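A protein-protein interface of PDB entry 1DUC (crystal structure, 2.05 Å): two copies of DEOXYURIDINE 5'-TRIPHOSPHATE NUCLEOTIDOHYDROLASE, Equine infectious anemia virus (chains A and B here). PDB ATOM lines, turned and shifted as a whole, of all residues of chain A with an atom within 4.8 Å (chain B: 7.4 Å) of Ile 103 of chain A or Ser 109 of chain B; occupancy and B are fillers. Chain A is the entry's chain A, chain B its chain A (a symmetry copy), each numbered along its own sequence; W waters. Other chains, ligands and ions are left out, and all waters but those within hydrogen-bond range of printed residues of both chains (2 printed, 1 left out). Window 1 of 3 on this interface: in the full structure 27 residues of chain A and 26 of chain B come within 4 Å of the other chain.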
ATOM      1  N   LYS A  12     -16.610   2.585  22.976  1.00  0.00           N
ATOM      2  CA  LYS A  12     -18.031   2.589  23.332  1.00  0.00           C
ATOM      3  C   LYS A  12     -18.333   3.793  24.224  1.00  0.00           C
ATOM      4  O   LYS A  12     -17.371   4.265  24.844  1.00  0.00           O
ATOM      5  CB  LYS A  12     -18.308   1.271  24.128  1.00  0.00           C
ATOM      6  CG  LYS A  12     -17.389   1.170  25.357  1.00  0.00           C
ATOM      7  CD  LYS A  12     -17.675  -0.133  26.121  1.00  0.00           C
ATOM      8  CE  LYS A  12     -19.042  -0.264  26.774  1.00  0.00           C
ATOM      9  NZ  LYS A  12     -19.226   0.722  27.925  1.00  0.00           N
ATOM     10  N   ALA A  17     -23.480  -1.350  27.519  1.00  0.00           N
ATOM     11  CA  ALA A  17     -22.847  -2.509  28.136  1.00  0.00           C
ATOM     12  C   ALA A  17     -21.679  -3.044  27.357  1.00  0.00           C
ATOM     13  O   ALA A  17     -20.867  -3.804  27.971  1.00  0.00           O
ATOM     14  CB  ALA A  17     -23.958  -3.638  28.189  1.00  0.00           C
ATOM     15  N   GLY A  18     -21.666  -2.893  26.042  1.00  0.00           N
ATOM     16  CA  GLY A  18     -20.728  -3.687  25.228  1.00  0.00           C
ATOM     17  C   GLY A  18     -20.086  -2.783  24.145  1.00  0.00           C
ATOM     18  O   GLY A  18     -20.566  -1.702  23.839  1.00  0.00           O
ATOM     19  N   PHE A  19     -19.039  -3.287  23.548  1.00  0.00           N
ATOM     20  CA  PHE A  19     -18.363  -2.677  22.410  1.00  0.00           C
ATOM     21  C   PHE A  19     -19.059  -3.272  21.171  1.00  0.00           C
ATOM     22  O   PHE A  19     -19.121  -4.499  21.041  1.00  0.00           O
ATOM     23  CB  PHE A  19     -16.906  -3.129  22.408  1.00  0.00           C
ATOM     24  CG  PHE A  19     -16.076  -2.717  23.594  1.00  0.00           C
ATOM     25  CD1 PHE A  19     -16.005  -3.500  24.726  1.00  0.00           C
ATOM     26  CD2 PHE A  19     -15.384  -1.506  23.561  1.00  0.00           C
ATOM     27  CE1 PHE A  19     -15.276  -3.115  25.844  1.00  0.00           C
ATOM     28  CE2 PHE A  19     -14.614  -1.118  24.675  1.00  0.00           C
ATOM     29  CZ  PHE A  19     -14.550  -1.902  25.806  1.00  0.00           C
ATOM     30  N   PHE A  50     -14.323 -13.107  31.396  1.00  0.00           N
ATOM     31  CA  PHE A  50     -14.493 -13.739  30.078  1.00  0.00           C
ATOM     32  C   PHE A  50     -15.155 -12.672  29.208  1.00  0.00           C
ATOM     33  O   PHE A  50     -15.771 -11.751  29.761  1.00  0.00           O
ATOM     34  CB  PHE A  50     -15.299 -15.047  30.074  1.00  0.00           C
ATOM     35  CG  PHE A  50     -16.740 -14.966  30.491  1.00  0.00           C
ATOM     36  CD1 PHE A  50     -17.080 -14.858  31.832  1.00  0.00           C
ATOM     37  CD2 PHE A  50     -17.760 -14.998  29.549  1.00  0.00           C
ATOM     38  CE1 PHE A  50     -18.422 -14.787  32.218  1.00  0.00           C
ATOM     39  CE2 PHE A  50     -19.104 -14.956  29.928  1.00  0.00           C
ATOM     40  CZ  PHE A  50     -19.431 -14.825  31.273  1.00  0.00           C
ATOM     41  N   GLY A  51     -15.070 -12.786  27.920  1.00  0.00           N
ATOM     42  CA  GLY A  51     -15.812 -11.919  27.018  1.00  0.00           C
ATOM     43  C   GLY A  51     -17.071 -12.648  26.515  1.00  0.00           C
ATOM     44  O   GLY A  51     -17.036 -13.855  26.255  1.00  0.00           O
ATOM     45  N   TRP A  52     -18.143 -11.883  26.280  1.00  0.00           N
ATOM     46  CA  TRP A  52     -19.403 -12.487  25.858  1.00  0.00           C
ATOM     47  C   TRP A  52     -19.795 -11.708  24.563  1.00  0.00           C
ATOM     48  O   TRP A  52     -20.025 -10.501  24.617  1.00  0.00           O
ATOM     49  CB  TRP A  52     -20.502 -12.327  26.894  1.00  0.00           C
ATOM     50  CG  TRP A  52     -21.875 -12.861  26.538  1.00  0.00           C
ATOM     51  CD1 TRP A  52     -22.192 -13.821  25.645  1.00  0.00           C
ATOM     52  CD2 TRP A  52     -23.132 -12.416  27.076  1.00  0.00           C
ATOM     53  NE1 TRP A  52     -23.559 -14.035  25.610  1.00  0.00           N
ATOM     54  CE2 TRP A  52     -24.139 -13.170  26.488  1.00  0.00           C
ATOM     55  CE3 TRP A  52     -23.445 -11.421  28.029  1.00  0.00           C
ATOM     56  CZ2 TRP A  52     -25.503 -13.033  26.810  1.00  0.00           C
ATOM     57  CZ3 TRP A  52     -24.785 -11.253  28.353  1.00  0.00           C
ATOM     58  CH2 TRP A  52     -25.765 -12.047  27.752  1.00  0.00           C
ATOM     59  N   THR A  54     -22.543 -11.169  21.901  1.00  0.00           N
ATOM     60  CA  THR A  54     -23.980 -11.414  21.854  1.00  0.00           C
ATOM     61  C   THR A  54     -24.629 -10.386  20.922  1.00  0.00           C
ATOM     62  O   THR A  54     -23.948  -9.626  20.191  1.00  0.00           O
ATOM     63  CB  THR A  54     -24.506 -11.422  23.282  1.00  0.00           C
ATOM     64  OG1 THR A  54     -25.881 -11.854  23.230  1.00  0.00           O
ATOM     65  CG2 THR A  54     -24.550 -10.043  23.966  1.00  0.00           C
ATOM     66  N   GLN A 101     -22.026  -7.430  19.756  1.00  0.00           N
ATOM     67  CA  GLN A 101     -21.336  -6.625  20.747  1.00  0.00           C
ATOM     68  C   GLN A 101     -20.628  -7.551  21.734  1.00  0.00           C
ATOM     69  O   GLN A 101     -20.999  -8.699  21.878  1.00  0.00           O
ATOM     70  CB  GLN A 101     -22.283  -5.683  21.519  1.00  0.00           C
ATOM     71  CG  GLN A 101     -23.433  -6.424  22.234  1.00  0.00           C
ATOM     72  CD  GLN A 101     -24.339  -5.464  23.000  1.00  0.00           C
ATOM     73  OE1 GLN A 101     -23.908  -4.528  23.663  1.00  0.00           O
ATOM     74  NE2 GLN A 101     -25.633  -5.650  22.936  1.00  0.00           N
ATOM     75  N   LEU A 102     -19.575  -7.003  22.329  1.00  0.00           N
ATOM     76  CA  LEU A 102     -18.729  -7.778  23.196  1.00  0.00           C
ATOM     77  C   LEU A 102     -18.875  -7.180  24.600  1.00  0.00           C
ATOM     78  O   LEU A 102     -18.710  -5.965  24.747  1.00  0.00           O
ATOM     79  CB  LEU A 102     -17.268  -7.555  22.726  1.00  0.00           C
ATOM     80  CG  LEU A 102     -16.257  -8.105  23.754  1.00  0.00           C
ATOM     81  CD1 LEU A 102     -16.268  -9.621  23.844  1.00  0.00           C
ATOM     82  CD2 LEU A 102     -14.855  -7.650  23.279  1.00  0.00           C
ATOM     83  N   ILE A 103     -19.266  -8.025  25.555  1.00  0.00           N
ATOM     84  CA  ILE A 103     -19.463  -7.493  26.909  1.00  0.00           C
ATOM     85  C   ILE A 103     -18.461  -8.223  27.779  1.00  0.00           C
ATOM     86  O   ILE A 103     -18.271  -9.475  27.562  1.00  0.00           O
ATOM     87  CB  ILE A 103     -20.924  -7.857  27.349  1.00  0.00           C
ATOM     88  CG1 ILE A 103     -21.953  -7.133  26.473  1.00  0.00           C
ATOM     89  CG2 ILE A 103     -21.100  -7.459  28.843  1.00  0.00           C
ATOM     90  CD1 ILE A 103     -23.401  -7.585  26.724  1.00  0.00           C
ATOM     91  N   ILE A 104     -17.838  -7.566  28.762  1.00  0.00           N
ATOM     92  CA  ILE A 104     -16.822  -8.279  29.598  1.00  0.00           C
ATOM     93  C   ILE A 104     -17.464  -8.594  30.940  1.00  0.00           C
ATOM     94  O   ILE A 104     -18.020  -7.705  31.583  1.00  0.00           O
ATOM     95  CB  ILE A 104     -15.540  -7.414  29.811  1.00  0.00           C
ATOM     96  CG1 ILE A 104     -14.953  -6.996  28.454  1.00  0.00           C
ATOM     97  CG2 ILE A 104     -14.488  -8.103  30.669  1.00  0.00           C
ATOM     98  CD1 ILE A 104     -14.545  -8.177  27.562  1.00  0.00           C
ATOM     99  N   LEU A 105     -17.431  -9.858  31.375  1.00  0.00           N
ATOM    100  CA  LEU A 105     -18.091 -10.226  32.636  1.00  0.00           C
ATOM    101  C   LEU A 105     -17.045 -10.921  33.533  1.00  0.00           C
ATOM    102  O   LEU A 105     -16.067 -11.434  33.026  1.00  0.00           O
ATOM    103  CB  LEU A 105     -19.212 -11.250  32.404  1.00  0.00           C
ATOM    104  CG  LEU A 105     -20.391 -10.754  31.537  1.00  0.00           C
ATOM    105  CD1 LEU A 105     -21.379 -11.861  31.189  1.00  0.00           C
ATOM    106  CD2 LEU A 105     -21.228  -9.760  32.356  1.00  0.00           C
ATOM    107  N   ASN B  48     -22.344   0.767  35.347  1.00  0.00           N
ATOM    108  CA  ASN B  48     -21.653  -0.465  34.966  1.00  0.00           C
ATOM    109  C   ASN B  48     -22.536  -1.685  35.216  1.00  0.00           C
ATOM    110  O   ASN B  48     -22.018  -2.785  35.314  1.00  0.00           O
ATOM    111  CB  ASN B  48     -20.302  -0.667  35.720  1.00  0.00           C
ATOM    112  CG  ASN B  48     -19.431   0.529  35.242  1.00  0.00           C
ATOM    113  OD1 ASN B  48     -19.459   0.957  34.082  1.00  0.00           O
ATOM    114  ND2 ASN B  48     -18.703   1.092  36.176  1.00  0.00           N
ATOM    115  N   PHE B  50     -26.310  -3.819  33.756  1.00  0.00           N
ATOM    116  CA  PHE B  50     -27.151  -3.889  32.551  1.00  0.00           C
ATOM    117  C   PHE B  50     -28.256  -4.885  32.895  1.00  0.00           C
ATOM    118  O   PHE B  50     -28.062  -5.699  33.807  1.00  0.00           O
ATOM    119  CB  PHE B  50     -26.419  -4.287  31.260  1.00  0.00           C
ATOM    120  CG  PHE B  50     -25.811  -5.659  31.211  1.00  0.00           C
ATOM    121  CD1 PHE B  50     -24.619  -5.927  31.870  1.00  0.00           C
ATOM    122  CD2 PHE B  50     -26.424  -6.689  30.508  1.00  0.00           C
ATOM    123  CE1 PHE B  50     -24.053  -7.204  31.819  1.00  0.00           C
ATOM    124  CE2 PHE B  50     -25.851  -7.960  30.429  1.00  0.00           C
ATOM    125  CZ  PHE B  50     -24.669  -8.221  31.112  1.00  0.00           C
ATOM    126  N   ILE B  70     -30.228  -7.273  25.529  1.00  0.00           N
ATOM    127  CA  ILE B  70     -29.246  -6.582  26.383  1.00  0.00           C
ATOM    128  C   ILE B  70     -29.816  -5.171  26.644  1.00  0.00           C
ATOM    129  O   ILE B  70     -30.041  -4.436  25.683  1.00  0.00           O
ATOM    130  CB  ILE B  70     -27.858  -6.505  25.731  1.00  0.00           C
ATOM    131  CG1 ILE B  70     -27.258  -7.907  25.430  1.00  0.00           C
ATOM    132  CG2 ILE B  70     -26.973  -5.602  26.613  1.00  0.00           C
ATOM    133  CD1 ILE B  70     -27.115  -8.784  26.702  1.00  0.00           C
ATOM    134  N   ILE B  71     -30.116  -4.849  27.886  1.00  0.00           N
ATOM    135  CA  ILE B  71     -30.750  -3.541  28.218  1.00  0.00           C
ATOM    136  C   ILE B  71     -29.682  -2.622  28.829  1.00  0.00           C
ATOM    137  O   ILE B  71     -29.181  -2.928  29.923  1.00  0.00           O
ATOM    138  CB  ILE B  71     -31.899  -3.674  29.209  1.00  0.00           C
ATOM    139  CG1 ILE B  71     -32.891  -4.807  28.879  1.00  0.00           C
ATOM    140  CG2 ILE B  71     -32.678  -2.320  29.297  1.00  0.00           C
ATOM    141  CD1 ILE B  71     -33.471  -4.678  27.453  1.00  0.00           C
ATOM    142  N   ASP B  72     -29.207  -1.621  28.070  1.00  0.00           N
ATOM    143  CA  ASP B  72     -28.077  -0.854  28.507  1.00  0.00           C
ATOM    144  C   ASP B  72     -28.484   0.077  29.678  1.00  0.00           C
ATOM    145  O   ASP B  72     -29.621   0.498  29.775  1.00  0.00           O
ATOM    146  CB  ASP B  72     -27.569   0.120  27.382  1.00  0.00           C
ATOM    147  CG  ASP B  72     -27.122  -0.731  26.196  1.00  0.00           C
ATOM    148  OD1 ASP B  72     -26.063  -1.370  26.260  1.00  0.00           O
ATOM    149  OD2 ASP B  72     -27.832  -0.820  25.171  1.00  0.00           O
ATOM    150  N   LEU B 105     -27.166  -7.719  35.823  1.00  0.00           N
ATOM    151  CA  LEU B 105     -25.772  -8.161  35.968  1.00  0.00           C
ATOM    152  C   LEU B 105     -24.880  -6.902  36.038  1.00  0.00           C
ATOM    153  O   LEU B 105     -25.287  -5.855  35.574  1.00  0.00           O
ATOM    154  CB  LEU B 105     -25.304  -8.956  34.740  1.00  0.00           C
ATOM    155  CG  LEU B 105     -26.055 -10.282  34.487  1.00  0.00           C
ATOM    156  CD1 LEU B 105     -25.678 -10.935  33.162  1.00  0.00           C
ATOM    157  CD2 LEU B 105     -25.617 -11.312  35.540  1.00  0.00           C
ATOM    158  N   GLN B 106     -23.644  -7.047  36.445  1.00  0.00           N
ATOM    159  CA  GLN B 106     -22.648  -5.988  36.302  1.00  0.00           C
ATOM    160  C   GLN B 106     -21.691  -6.361  35.212  1.00  0.00           C
ATOM    161  O   GLN B 106     -21.390  -7.555  35.160  1.00  0.00           O
ATOM    162  CB  GLN B 106     -21.747  -5.989  37.566  1.00  0.00           C
ATOM    163  CG  GLN B 106     -22.512  -5.411  38.764  1.00  0.00           C
ATOM    164  CD  GLN B 106     -21.524  -5.226  39.929  1.00  0.00           C
ATOM    165  OE1 GLN B 106     -20.298  -5.338  39.808  1.00  0.00           O
ATOM    166  NE2 GLN B 106     -22.069  -4.951  41.101  1.00  0.00           N
ATOM    167  N   HIS B 107     -21.251  -5.423  34.382  1.00  0.00           N
ATOM    168  CA  HIS B 107     -20.239  -5.760  33.394  1.00  0.00           C
ATOM    169  C   HIS B 107     -18.958  -5.000  33.779  1.00  0.00           C
ATOM    170  O   HIS B 107     -18.982  -4.171  34.700  1.00  0.00           O
ATOM    171  CB  HIS B 107     -20.702  -5.288  32.014  1.00  0.00           C
ATOM    172  CG  HIS B 107     -20.721  -3.788  31.845  1.00  0.00           C
ATOM    173  ND1 HIS B 107     -19.629  -3.008  31.683  1.00  0.00           N
ATOM    174  CD2 HIS B 107     -21.803  -2.950  31.840  1.00  0.00           C
ATOM    175  CE1 HIS B 107     -20.019  -1.745  31.548  1.00  0.00           C
ATOM    176  NE2 HIS B 107     -21.367  -1.678  31.632  1.00  0.00           N
ATOM    177  N   HIS B 108     -17.858  -5.442  33.194  1.00  0.00           N
ATOM    178  CA  HIS B 108     -16.575  -4.719  33.388  1.00  0.00           C
ATOM    179  C   HIS B 108     -16.116  -4.220  32.048  1.00  0.00           C
ATOM    180  O   HIS B 108     -14.886  -4.324  31.714  1.00  0.00           O
ATOM    181  CB  HIS B 108     -15.574  -5.756  34.060  1.00  0.00           C
ATOM    182  CG  HIS B 108     -16.238  -6.320  35.299  1.00  0.00           C
ATOM    183  ND1 HIS B 108     -16.036  -5.777  36.554  1.00  0.00           N
ATOM    184  CD2 HIS B 108     -17.159  -7.313  35.482  1.00  0.00           C
ATOM    185  CE1 HIS B 108     -16.795  -6.443  37.436  1.00  0.00           C
ATOM    186  NE2 HIS B 108     -17.505  -7.362  36.815  1.00  0.00           N
ATOM    187  N   SER B 109     -16.980  -3.744  31.143  1.00  0.00           N
ATOM    188  CA  SER B 109     -16.604  -3.315  29.797  1.00  0.00           C
ATOM    189  C   SER B 109     -16.036  -1.903  29.664  1.00  0.00           C
ATOM    190  O   SER B 109     -16.624  -1.057  28.954  1.00  0.00           O
ATOM    191  CB  SER B 109     -17.796  -3.407  28.795  1.00  0.00           C
ATOM    192  OG  SER B 109     -18.403  -4.725  28.809  1.00  0.00           O
ATOM    193  N   ASN B 110     -14.977  -1.503  30.283  1.00  0.00           N
ATOM    194  CA  ASN B 110     -14.601  -0.092  30.532  1.00  0.00           C
ATOM    195  C   ASN B 110     -13.145  -0.181  31.000  1.00  0.00           C
ATOM    196  O   ASN B 110     -12.533  -1.276  31.006  1.00  0.00           O
ATOM    197  CB  ASN B 110     -15.585   0.571  31.518  1.00  0.00           C
ATOM    198  CG  ASN B 110     -16.875   1.122  30.937  1.00  0.00           C
ATOM    199  OD1 ASN B 110     -16.916   1.388  29.722  1.00  0.00           O
ATOM    200  ND2 ASN B 110     -17.982   1.339  31.652  1.00  0.00           N
ATOM    201  N   SER B 111     -12.466   0.944  31.255  1.00  0.00           N
ATOM    202  CA  SER B 111     -11.087   0.992  31.707  1.00  0.00           C
ATOM    203  C   SER B 111     -10.124   0.129  30.894  1.00  0.00           C
ATOM    204  O   SER B 111      -9.430  -0.790  31.335  1.00  0.00           O
ATOM    205  CB  SER B 111     -10.943   0.609  33.172  1.00  0.00           C
ATOM    206  OG  SER B 111     -11.997  -0.221  33.605  1.00  0.00           O
ATOM    207  N   ARG B 112      -9.980   0.544  29.647  1.00  0.00           N
ATOM    208  CA  ARG B 112      -9.143  -0.107  28.659  1.00  0.00           C
ATOM    209  C   ARG B 112      -7.705  -0.098  29.199  1.00  0.00           C
ATOM    210  O   ARG B 112      -7.300   0.898  29.807  1.00  0.00           O
ATOM    211  CB  ARG B 112      -9.178   0.595  27.297  1.00  0.00           C
ATOM    212  CG  ARG B 112      -8.239   0.003  26.252  1.00  0.00           C
ATOM    213  CD  ARG B 112      -8.251   0.768  24.921  1.00  0.00           C
ATOM    214  NE  ARG B 112      -7.532  -0.031  23.905  1.00  0.00           N
ATOM    215  CZ  ARG B 112      -7.473   0.284  22.612  1.00  0.00           C
ATOM    216  NH1 ARG B 112      -8.096   1.395  22.198  1.00  0.00           N
ATOM    217  NH2 ARG B 112      -6.824  -0.482  21.729  1.00  0.00           N
HETATM  218  O   HOH W   1     -24.459  -2.022  24.236  1.00  0.00           O
HETATM  219  O   HOH W   2     -27.718  -3.423  24.134  1.00  0.00           O
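Of the printed residues of chain B, Ile 103 of chain A touches Ile 70, His 107 and Ser 109.
Of the printed residues of chain A, Ser 109 of chain B touches Lys 12 (3.2 Å), Ala 17 (2.8 Å), Phe 19 (3.9 Å), Ile 103 (3.5 Å) and Ile 104 (2.9 Å).
Printed residues of chain A within 4 Å of Asp 72 of chain B: Ala 17 (2.9 Å).
Printed residues of chain A within 4 Å of Asn 110 of chain B: Lys 12 (3.0 Å).
The nearest printed residue of chain A that does not touch Phe 50 of chain B is Trp 52 of chain A (4.04 Å).
Leu 105 of chain A touches Phe 50 of chain B, but with the chains exchanged Phe 50 of chain A does not touch Leu 105 of chain B (7.6 Å).
2 positions are printed for both chains.
Of the 19 pairs that touch across the chains among the printed residues, none has its exchanged pair printed and touching as well.
Ala 17 of chain A touches Phe 50 of chain B.
Ala 17 of chain A touches Ile 70 of chain B (CB to CG2, 3.9 Å).
His 107 of chain B touches Ala 17 of chain A.
Ser 109 of chain B touches Phe 19 of chain A.
Ile 70 of chain B touches Thr 54 of chain A.
Ile 70 of chain B touches Gln 101 of chain A (CB to NE2, 3.7 Å).
CD1 of Ile 103 of chain A touches CD1 of Ile 70 of chain B, 3.9 Å away.
Ser 109 of chain B touches Ile 103 of chain A.
Phe 50 of chain B touches Leu 105 of chain A (CE1 to CD2, 3.8 Å).
O of Gln 106 of chain B touches CD2 of Leu 105 of chain A, 3.6 Å away.
Water W1 lies within hydrogen-bond range of OE1 of Gln 101 of chain A (2.6 Å), OD1 of Asp 72 of chain B (2.7 Å), N of Gly 18 of chain A (3.4 Å) and N of Ala 17 of chain A (3.5 Å).
Water W2 lies within hydrogen-bond range of the side-chain carboxylate (OD2) of Asp 72 of chain B, the backbone carbonyl oxygen (O) of Ile 70 of chain B and the side-chain amide nitrogen (NE2) of Gln 101 of chain A.
N of Leu 102 of chain A lies within hydrogen-bond range of O of Phe 19 of chain A, 2.9 Å away.
N of Phe 50 of chain A is in hydrogen-bond range of O of Leu 105 of chain A (2.9 Å).
The backbone NH (N) of Trp 52 of chain A sits at hydrogen-bond distance from the backbone carbonyl oxygen (O) of Ile 103 of chain A (2.7 Å).
The backbone NH (N) of Thr 54 of chain A lies within hydrogen-bond range of the backbone carbonyl oxygen (O) of Gln 101 of chain A, at 2.9 Å.
N of Phe 50 of chain B lies within hydrogen-bond range of O of Leu 105 of chain B, 2.9 Å away.
A ring nitrogen (ND1) of His 107 of chain B sits at hydrogen-bond distance from the backbone NH of Ser 109 of chain B (2.8 Å).
Of the 13 printed residues of chain B, 8 touch a printed residue of chain A.
Hydrophobic or aromatic side chains of chain B that line the printed part of chain A: Phe 50, Ile 70, His 107 and His 108.
Of the 13 printed residues of chain A, 9 touch a printed residue of chain B.
Hydrophobic or aromatic side chains of chain A that line the printed part of chain B: Ala 17, Phe 19, Trp 52, Ile 103, Ile 104 and Leu 105.
The side-chain amino group (NZ) of Lys 12 of chain A lies close to the backbone carbonyl oxygen (O) of Ser 109 of chain B, 3.3 Å away.
The side-chain amide oxygen (OD1) of Asn 110 of chain B sits at hydrogen-bond distance from the side-chain amino group (NZ) of Lys 12 of chain A (3.0 Å).
OD1 of Asp 72 of chain B sits at hydrogen-bond distance from N of Ala 17 of chain A (2.9 Å).
O of Ala 17 of chain A lies within hydrogen-bond range of OG of Ser 109 of chain B, 2.8 Å away.
The backbone carbonyl oxygen (O) of Ile 104 of chain A sits at hydrogen-bond distance from the backbone NH (N) of His 108 of chain B.
The side-chain hydroxyl of Ser 109 of chain B sits at hydrogen-bond distance from the backbone NH of Ile 104 of chain A, at 2.9 Å.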
